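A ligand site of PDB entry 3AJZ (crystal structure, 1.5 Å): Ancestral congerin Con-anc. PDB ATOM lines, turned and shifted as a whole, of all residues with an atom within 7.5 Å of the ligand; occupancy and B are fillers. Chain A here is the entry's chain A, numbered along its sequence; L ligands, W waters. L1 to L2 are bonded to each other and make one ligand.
The side-chain carboxylate (OE1) of Glu 72 lies within salt-bridge range of the guanidinium group (NH1) of Arg 74 (2.7 Å).
The guanidinium group (NE) of Arg 49 is in salt-bridge range of the side-chain carboxylate (OD2) of Asp 47.
N of His 45 lies within hydrogen-bond range of O of Asn 62 (2.8 Å).
ND1 of His 45 is in hydrogen-bond range of OD1 of Asn 34 (2.8 Å).
The side-chain amide nitrogen of Asn 62 lies within hydrogen-bond range of the backbone carbonyl oxygen of Gln 70 (2.8 Å).
O of Gln 71 lies close to OD1 of Asn 62 (3.1 Å).
The side-chain carboxylate (OD2) of Asp 47 is in salt-bridge range of the guanidinium group (NH2) of Arg 30, at 2.8 Å.
The backbone NH (N) of Asp 47 sits at hydrogen-bond distance from the backbone carbonyl oxygen (O) of Val 60 (2.8 Å).
OE2 of Glu 72 is in hydrogen-bond range of O3 of LIG L1, at 2.6 Å.
An oxygen (O1) of LG2 L2 lies within hydrogen-bond range of the side-chain hydroxyl (OH) of Tyr 52, 2.8 Å away.
The guanidinium group (NH2) of Arg 49 lies within hydrogen-bond range of an oxygen (O3) of LIG L1.
A ring nitrogen (NE2) of His 45 lies within hydrogen-bond range of an oxygen (O3) of LG2 L2, at 2.9 Å.
An oxygen (O5) of LG2 L2 sits at hydrogen-bond distance from the side-chain amide nitrogen (ND2) of Asn 62.
The guanidinium group (NH2) of Arg 30 lies within hydrogen-bond range of an oxygen (O2) of LG2 L2, 3.0 Å away.
An oxygen (O3) of LG2 L2 sits at hydrogen-bond distance from the side-chain carboxylate of Asp 47 (3.2 Å).
Water W1 lies within hydrogen-bond range of the side-chain carboxylate (OE1) of Glu 72, an oxygen (O2) of LIG L1 and the guanidinium group (NH2) of Arg 74.
Water W3 lies within hydrogen-bond range of OD2 of Asp 55 (2.8 Å), N of Ala 54 (2.9 Å) and O2 of LIG L1 (3.0 Å).
Water W4 bridges O5 of LG2 L2 and OE2 of Glu 72.
Residues that only touch the ligand: Trp 69 and Arg 74.
Hydrophobic or aromatic side chains within 4 Å of the ligand: His 45, Tyr 52 and Trp 69.
Within 4 Å of the ligand: Arg 30, His 45, Asp 47, Arg 49, Tyr 52, Asn 62, Trp 69, Glu 72 and Arg 74.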
ATOM      1  N   ARG A  30      18.521   5.384 -15.184  1.00  0.00           N
ATOM      2  CA  ARG A  30      19.438   4.287 -15.505  1.00  0.00           C
ATOM      3  C   ARG A  30      20.826   4.639 -14.996  1.00  0.00           C
ATOM      4  O   ARG A  30      21.174   5.816 -14.796  1.00  0.00           O
ATOM      5  CB  ARG A  30      19.496   4.067 -17.016  1.00  0.00           C
ATOM      6  CG  ARG A  30      20.095   5.278 -17.778  1.00  0.00           C
ATOM      7  CD  ARG A  30      20.263   4.927 -19.243  1.00  0.00           C
ATOM      8  NE  ARG A  30      20.760   6.065 -20.021  1.00  0.00           N
ATOM      9  CZ  ARG A  30      21.557   5.960 -21.083  1.00  0.00           C
ATOM     10  NH1 ARG A  30      21.896   7.049 -21.747  1.00  0.00           N
ATOM     11  NH2 ARG A  30      21.951   4.763 -21.534  1.00  0.00           N
ATOM     12  N   SER A  32      25.088   2.933 -15.701  1.00  0.00           N
ATOM     13  CA  SER A  32      25.907   1.874 -16.320  1.00  0.00           C
ATOM     14  C   SER A  32      27.271   1.632 -15.687  1.00  0.00           C
ATOM     15  O   SER A  32      27.892   2.540 -15.130  1.00  0.00           O
ATOM     16  CB  SER A  32      26.078   2.094 -17.843  1.00  0.00           C
ATOM     17  OG  SER A  32      26.704   3.343 -18.062  1.00  0.00           O
ATOM     18  N   ASN A  34      30.998   0.285 -17.029  1.00  0.00           N
ATOM     19  CA  ASN A  34      31.655   0.303 -18.353  1.00  0.00           C
ATOM     20  C   ASN A  34      33.071  -0.143 -18.164  1.00  0.00           C
ATOM     21  O   ASN A  34      33.824   0.581 -17.514  1.00  0.00           O
ATOM     22  CB  ASN A  34      31.636   1.720 -18.911  1.00  0.00           C
ATOM     23  CG  ASN A  34      30.240   2.227 -19.098  1.00  0.00           C
ATOM     24  OD1 ASN A  34      29.644   1.997 -20.151  1.00  0.00           O
ATOM     25  ND2 ASN A  34      29.704   2.921 -18.101  1.00  0.00           N
ATOM     26  N   HIS A  45      29.529  -2.872 -21.535  1.00  0.00           N
ATOM     27  CA  HIS A  45      28.625  -1.837 -21.046  1.00  0.00           C
ATOM     28  C   HIS A  45      27.427  -2.530 -20.478  1.00  0.00           C
ATOM     29  O   HIS A  45      26.761  -3.307 -21.176  1.00  0.00           O
ATOM     30  CB  HIS A  45      28.222  -0.963 -22.237  1.00  0.00           C
ATOM     31  CG  HIS A  45      27.085  -0.010 -21.967  1.00  0.00           C
ATOM     32  ND1 HIS A  45      27.217   1.149 -21.227  1.00  0.00           N
ATOM     33  CD2 HIS A  45      25.816   0.003 -22.464  1.00  0.00           C
ATOM     34  CE1 HIS A  45      26.073   1.826 -21.266  1.00  0.00           C
ATOM     35  NE2 HIS A  45      25.202   1.144 -21.994  1.00  0.00           N
ATOM     36  N   ILE A  46      27.146  -2.286 -19.204  1.00  0.00           N
ATOM     37  CA  ILE A  46      25.993  -2.907 -18.538  1.00  0.00           C
ATOM     38  C   ILE A  46      25.102  -1.763 -18.118  1.00  0.00           C
ATOM     39  O   ILE A  46      25.453  -1.034 -17.193  1.00  0.00           O
ATOM     40  CB  ILE A  46      26.441  -3.677 -17.262  1.00  0.00           C
ATOM     41  CG1 ILE A  46      27.652  -4.587 -17.536  1.00  0.00           C
ATOM     42  CG2 ILE A  46      25.252  -4.472 -16.730  1.00  0.00           C
ATOM     43  CD1 ILE A  46      28.324  -5.065 -16.240  1.00  0.00           C
ATOM     44  N   ASP A  47      23.991  -1.583 -18.821  1.00  0.00           N
ATOM     45  CA  ASP A  47      23.104  -0.441 -18.573  1.00  0.00           C
ATOM     46  C   ASP A  47      21.910  -0.923 -17.788  1.00  0.00           C
ATOM     47  O   ASP A  47      21.100  -1.714 -18.286  1.00  0.00           O
ATOM     48  CB  ASP A  47      22.650   0.192 -19.906  1.00  0.00           C
ATOM     49  CG  ASP A  47      22.303   1.663 -19.779  1.00  0.00           C
ATOM     50  OD1 ASP A  47      22.790   2.317 -18.835  1.00  0.00           O
ATOM     51  OD2 ASP A  47      21.527   2.147 -20.622  1.00  0.00           O
ATOM     52  N   ARG A  49      18.577  -0.226 -16.669  1.00  0.00           N
ATOM     53  CA  ARG A  49      17.501   0.702 -17.016  1.00  0.00           C
ATOM     54  C   ARG A  49      16.258   0.528 -16.168  1.00  0.00           C
ATOM     55  O   ARG A  49      15.465  -0.396 -16.393  1.00  0.00           O
ATOM     56  CB  ARG A  49      17.128   0.578 -18.510  1.00  0.00           C
ATOM     57  CG  ARG A  49      18.330   0.868 -19.376  1.00  0.00           C
ATOM     58  CD  ARG A  49      17.971   0.793 -20.853  1.00  0.00           C
ATOM     59  NE  ARG A  49      19.148   1.154 -21.621  1.00  0.00           N
ATOM     60  CZ  ARG A  49      19.197   1.267 -22.942  1.00  0.00           C
ATOM     61  NH1 ARG A  49      20.332   1.614 -23.525  1.00  0.00           N
ATOM     62  NH2 ARG A  49      18.119   1.004 -23.687  1.00  0.00           N
ATOM     63  N   TYR A  52      14.053   3.838 -19.361  1.00  0.00           N
ATOM     64  CA  TYR A  52      14.779   4.561 -20.374  1.00  0.00           C
ATOM     65  C   TYR A  52      14.349   4.027 -21.719  1.00  0.00           C
ATOM     66  O   TYR A  52      14.335   2.817 -21.939  1.00  0.00           O
ATOM     67  CB  TYR A  52      16.309   4.402 -20.197  1.00  0.00           C
ATOM     68  CG  TYR A  52      17.123   5.070 -21.300  1.00  0.00           C
ATOM     69  CD1 TYR A  52      17.474   6.417 -21.217  1.00  0.00           C
ATOM     70  CD2 TYR A  52      17.489   4.338 -22.418  1.00  0.00           C
ATOM     71  CE1 TYR A  52      18.191   7.032 -22.252  1.00  0.00           C
ATOM     72  CE2 TYR A  52      18.188   4.929 -23.451  1.00  0.00           C
ATOM     73  CZ  TYR A  52      18.551   6.268 -23.344  1.00  0.00           C
ATOM     74  OH  TYR A  52      19.233   6.838 -24.401  1.00  0.00           O
ATOM     75  N   GLY A  53      14.001   4.918 -22.639  1.00  0.00           N
ATOM     76  CA  GLY A  53      13.571   4.439 -23.968  1.00  0.00           C
ATOM     77  C   GLY A  53      12.347   3.544 -23.832  1.00  0.00           C
ATOM     78  O   GLY A  53      11.436   3.855 -23.089  1.00  0.00           O
ATOM     79  N   ALA A  54      12.361   2.401 -24.504  1.00  0.00           N
ATOM     80  CA  ALA A  54      11.232   1.455 -24.411  1.00  0.00           C
ATOM     81  C   ALA A  54      11.426   0.405 -23.316  1.00  0.00           C
ATOM     82  O   ALA A  54      10.647  -0.556 -23.195  1.00  0.00           O
ATOM     83  CB  ALA A  54      10.945   0.808 -25.777  1.00  0.00           C
ATOM     84  N   ASP A  55      12.466   0.607 -22.501  1.00  0.00           N
ATOM     85  CA  ASP A  55      12.870  -0.362 -21.501  1.00  0.00           C
ATOM     86  C   ASP A  55      12.444   0.049 -20.101  1.00  0.00           C
ATOM     87  O   ASP A  55      12.721   1.169 -19.667  1.00  0.00           O
ATOM     88  CB  ASP A  55      14.397  -0.540 -21.498  1.00  0.00           C
ATOM     89  CG  ASP A  55      14.904  -1.177 -22.780  1.00  0.00           C
ATOM     90  OD1 ASP A  55      14.447  -2.292 -23.106  1.00  0.00           O
ATOM     91  OD2 ASP A  55      15.731  -0.557 -23.492  1.00  0.00           O
ATOM     92  N   VAL A  60      20.344  -3.657 -20.255  1.00  0.00           N
ATOM     93  CA  VAL A  60      20.778  -3.671 -21.649  1.00  0.00           C
ATOM     94  C   VAL A  60      22.287  -3.751 -21.655  1.00  0.00           C
ATOM     95  O   VAL A  60      22.960  -2.916 -21.055  1.00  0.00           O
ATOM     96  CB  VAL A  60      20.282  -2.410 -22.377  1.00  0.00           C
ATOM     97  CG1 VAL A  60      20.866  -2.369 -23.789  1.00  0.00           C
ATOM     98  CG2 VAL A  60      18.742  -2.417 -22.383  1.00  0.00           C
ATOM     99  N   LEU A  61      22.803  -4.778 -22.311  1.00  0.00           N
ATOM    100  CA  LEU A  61      24.232  -5.007 -22.424  1.00  0.00           C
ATOM    101  C   LEU A  61      24.691  -4.712 -23.845  1.00  0.00           C
ATOM    102  O   LEU A  61      24.020  -5.054 -24.842  1.00  0.00           O
ATOM    103  CB  LEU A  61      24.621  -6.440 -22.016  1.00  0.00           C
ATOM    104  CG  LEU A  61      24.178  -6.769 -20.589  1.00  0.00           C
ATOM    105  CD1 LEU A  61      22.816  -7.495 -20.571  1.00  0.00           C
ATOM    106  CD2 LEU A  61      25.261  -7.577 -19.908  1.00  0.00           C
ATOM    107  N   ASN A  62      25.846  -4.105 -23.967  1.00  0.00           N
ATOM    108  CA  ASN A  62      26.424  -3.850 -25.269  1.00  0.00           C
ATOM    109  C   ASN A  62      27.935  -3.608 -25.143  1.00  0.00           C
ATOM    110  O   ASN A  62      28.526  -3.677 -24.061  1.00  0.00           O
ATOM    111  CB  ASN A  62      25.678  -2.687 -25.930  1.00  0.00           C
ATOM    112  CG  ASN A  62      25.715  -2.749 -27.471  1.00  0.00           C
ATOM    113  OD1 ASN A  62      26.390  -3.593 -28.070  1.00  0.00           O
ATOM    114  ND2 ASN A  62      24.937  -1.848 -28.109  1.00  0.00           N
ATOM    115  N   SER A  63      28.572  -3.366 -26.274  1.00  0.00           N
ATOM    116  CA  SER A  63      29.942  -2.952 -26.385  1.00  0.00           C
ATOM    117  C   SER A  63      30.018  -1.795 -27.360  1.00  0.00           C
ATOM    118  O   SER A  63      29.089  -1.596 -28.166  1.00  0.00           O
ATOM    119  CB  SER A  63      30.813  -4.110 -26.890  1.00  0.00           C
ATOM    120  OG  SER A  63      30.221  -4.684 -28.076  1.00  0.00           O
ATOM    121  N   MET A  64      31.094  -1.041 -27.279  1.00  0.00           N
ATOM    122  CA  MET A  64      31.324   0.120 -28.153  1.00  0.00           C
ATOM    123  C   MET A  64      32.709   0.021 -28.764  1.00  0.00           C
ATOM    124  O   MET A  64      33.707  -0.134 -28.057  1.00  0.00           O
ATOM    125  CB  MET A  64      31.181   1.413 -27.334  1.00  0.00           C
ATOM    126  CG  MET A  64      31.886   2.623 -27.991  1.00  0.00           C
ATOM    127  SD  MET A  64      31.746   4.125 -26.995  1.00  0.00           S
ATOM    128  CE  MET A  64      30.055   4.411 -27.148  1.00  0.00           C
ATOM    129  N   TRP A  69      28.108   1.975 -30.917  1.00  0.00           N
ATOM    130  CA  TRP A  69      27.482   0.836 -30.241  1.00  0.00           C
ATOM    131  C   TRP A  69      27.302  -0.353 -31.155  1.00  0.00           C
ATOM    132  O   TRP A  69      27.034  -0.193 -32.349  1.00  0.00           O
ATOM    133  CB  TRP A  69      26.159   1.244 -29.619  1.00  0.00           C
ATOM    134  CG  TRP A  69      26.338   2.239 -28.500  1.00  0.00           C
ATOM    135  CD1 TRP A  69      26.009   3.553 -28.527  1.00  0.00           C
ATOM    136  CD2 TRP A  69      26.903   1.987 -27.212  1.00  0.00           C
ATOM    137  NE1 TRP A  69      26.333   4.151 -27.332  1.00  0.00           N
ATOM    138  CE2 TRP A  69      26.886   3.210 -26.505  1.00  0.00           C
ATOM    139  CE3 TRP A  69      27.420   0.849 -26.592  1.00  0.00           C
ATOM    140  CZ2 TRP A  69      27.367   3.323 -25.178  1.00  0.00           C
ATOM    141  CZ3 TRP A  69      27.892   0.960 -25.270  1.00  0.00           C
ATOM    142  CH2 TRP A  69      27.860   2.181 -24.597  1.00  0.00           C
ATOM    143  N   GLN A  70      27.444  -1.551 -30.592  1.00  0.00           N
ATOM    144  CA  GLN A  70      27.264  -2.783 -31.340  1.00  0.00           C
ATOM    145  C   GLN A  70      25.871  -3.357 -31.058  1.00  0.00           C
ATOM    146  O   GLN A  70      24.936  -2.577 -30.805  1.00  0.00           O
ATOM    147  CB  GLN A  70      28.422  -3.756 -31.037  1.00  0.00           C
ATOM    148  CG  GLN A  70      29.816  -3.184 -31.360  1.00  0.00           C
ATOM    149  CD  GLN A  70      30.944  -4.271 -31.289  1.00  0.00           C
ATOM    150  OE1 GLN A  70      31.460  -4.612 -30.208  1.00  0.00           O
ATOM    151  NE2 GLN A  70      31.345  -4.778 -32.457  1.00  0.00           N
ATOM    152  N   GLN A  71      25.683  -4.670 -31.133  1.00  0.00           N
ATOM    153  CA  GLN A  71      24.347  -5.245 -30.974  1.00  0.00           C
ATOM    154  C   GLN A  71      23.970  -5.424 -29.498  1.00  0.00           C
ATOM    155  O   GLN A  71      24.697  -6.053 -28.694  1.00  0.00           O
ATOM    156  CB  GLN A  71      24.226  -6.586 -31.719  1.00  0.00           C
ATOM    157  CG  GLN A  71      22.817  -7.192 -31.667  1.00  0.00           C
ATOM    158  CD  GLN A  71      22.567  -8.241 -32.762  1.00  0.00           C
ATOM    159  OE1 GLN A  71      23.502  -8.801 -33.359  1.00  0.00           O
ATOM    160  NE2 GLN A  71      21.287  -8.510 -33.019  1.00  0.00           N
ATOM    161  N   GLU A  72      22.813  -4.905 -29.136  1.00  0.00           N
ATOM    162  CA  GLU A  72      22.292  -5.032 -27.779  1.00  0.00           C
ATOM    163  C   GLU A  72      21.847  -6.408 -27.431  1.00  0.00           C
ATOM    164  O   GLU A  72      21.354  -7.188 -28.291  1.00  0.00           O
ATOM    165  CB  GLU A  72      21.112  -4.078 -27.577  1.00  0.00           C
ATOM    166  CG  GLU A  72      21.533  -2.652 -27.631  1.00  0.00           C
ATOM    167  CD  GLU A  72      20.377  -1.651 -27.555  1.00  0.00           C
ATOM    168  OE1 GLU A  72      19.190  -2.047 -27.611  1.00  0.00           O
ATOM    169  OE2 GLU A  72      20.656  -0.441 -27.434  1.00  0.00           O
ATOM    170  N   GLN A  73      22.051  -6.738 -26.156  1.00  0.00           N
ATOM    171  CA  GLN A  73      21.461  -7.904 -25.555  1.00  0.00           C
ATOM    172  C   GLN A  73      20.721  -7.442 -24.325  1.00  0.00           C
ATOM    173  O   GLN A  73      21.039  -6.395 -23.747  1.00  0.00           O
ATOM    174  CB  GLN A  73      22.535  -8.923 -25.186  1.00  0.00           C
ATOM    175  CG  GLN A  73      23.287  -9.445 -26.432  1.00  0.00           C
ATOM    176  CD  GLN A  73      24.203 -10.633 -26.189  1.00  0.00           C
ATOM    177  OE1 GLN A  73      24.366 -11.166 -25.047  1.00  0.00           O
ATOM    178  NE2 GLN A  73      24.814 -11.082 -27.298  1.00  0.00           N
ATOM    179  N   ARG A  74      19.694  -8.180 -23.939  1.00  0.00           N
ATOM    180  CA  ARG A  74      18.851  -7.761 -22.822  1.00  0.00           C
ATOM    181  C   ARG A  74      18.699  -8.862 -21.819  1.00  0.00           C
ATOM    182  O   ARG A  74      18.699 -10.052 -22.175  1.00  0.00           O
ATOM    183  CB  ARG A  74      17.480  -7.286 -23.289  1.00  0.00           C
ATOM    184  CG  ARG A  74      17.509  -5.847 -23.839  1.00  0.00           C
ATOM    185  CD  ARG A  74      16.187  -5.376 -24.475  1.00  0.00           C
ATOM    186  NE  ARG A  74      16.210  -3.931 -24.704  1.00  0.00           N
ATOM    187  CZ  ARG A  74      16.974  -3.325 -25.610  1.00  0.00           C
ATOM    188  NH1 ARG A  74      17.748  -4.031 -26.421  1.00  0.00           N
ATOM    189  NH2 ARG A  74      16.970  -2.000 -25.678  1.00  0.00           N
HETATM  190  C1  LIG L   1      17.546   1.812 -28.300  1.00  0.00           C
HETATM  191  C2  LIG L   1      18.343   2.258 -27.070  1.00  0.00           C
HETATM  192  C3  LIG L   1      19.505   3.174 -27.438  1.00  0.00           C
HETATM  193  C4  LIG L   1      18.882   4.323 -28.248  1.00  0.00           C
HETATM  194  C5  LIG L   1      19.882   5.374 -28.718  1.00  0.00           C
HETATM  195  C6  LIG L   1      17.082   3.060 -29.039  1.00  0.00           C
HETATM  196  O1  LIG L   1      16.482   2.690 -30.255  1.00  0.00           O
HETATM  197  O2  LIG L   1      16.426   1.059 -27.908  1.00  0.00           O
HETATM  198  O3  LIG L   1      18.838   1.128 -26.373  1.00  0.00           O
HETATM  199  O4  LIG L   1      20.062   3.720 -26.261  1.00  0.00           O
HETATM  200  O5  LIG L   1      18.246   3.777 -29.390  1.00  0.00           O
HETATM  201  O6  LIG L   1      20.887   4.735 -29.469  1.00  0.00           O
HETATM  202  C1  LG2 L   2      21.497   3.638 -26.177  1.00  0.00           C
HETATM  203  C2  LG2 L   2      21.967   4.621 -25.090  1.00  0.00           C
HETATM  204  C3  LG2 L   2      23.469   4.491 -24.834  1.00  0.00           C
HETATM  205  C4  LG2 L   2      23.787   3.014 -24.553  1.00  0.00           C
HETATM  206  C5  LG2 L   2      23.299   2.205 -25.763  1.00  0.00           C
HETATM  207  C6  LG2 L   2      23.586   0.722 -25.591  1.00  0.00           C
HETATM  208  O1  LG2 L   2      21.648   5.972 -25.442  1.00  0.00           O
HETATM  209  O2  LG2 L   2      23.830   5.300 -23.750  1.00  0.00           O
HETATM  210  O3  LG2 L   2      23.164   2.635 -23.325  1.00  0.00           O
HETATM  211  O4  LG2 L   2      21.879   2.301 -25.922  1.00  0.00           O
HETATM  212  O5  LG2 L   2      23.229   0.016 -26.765  1.00  0.00           O
HETATM  213  O   HOH W   1      17.101  -1.358 -29.017  1.00  0.00           O
HETATM  214  O   HOH W   2      25.609   5.266 -21.504  1.00  0.00           O
HETATM  215  O   HOH W   3      14.836   1.228 -25.418  1.00  0.00           O
HETATM  216  O   HOH W   4      22.399   1.104 -29.578  1.00  0.00           O
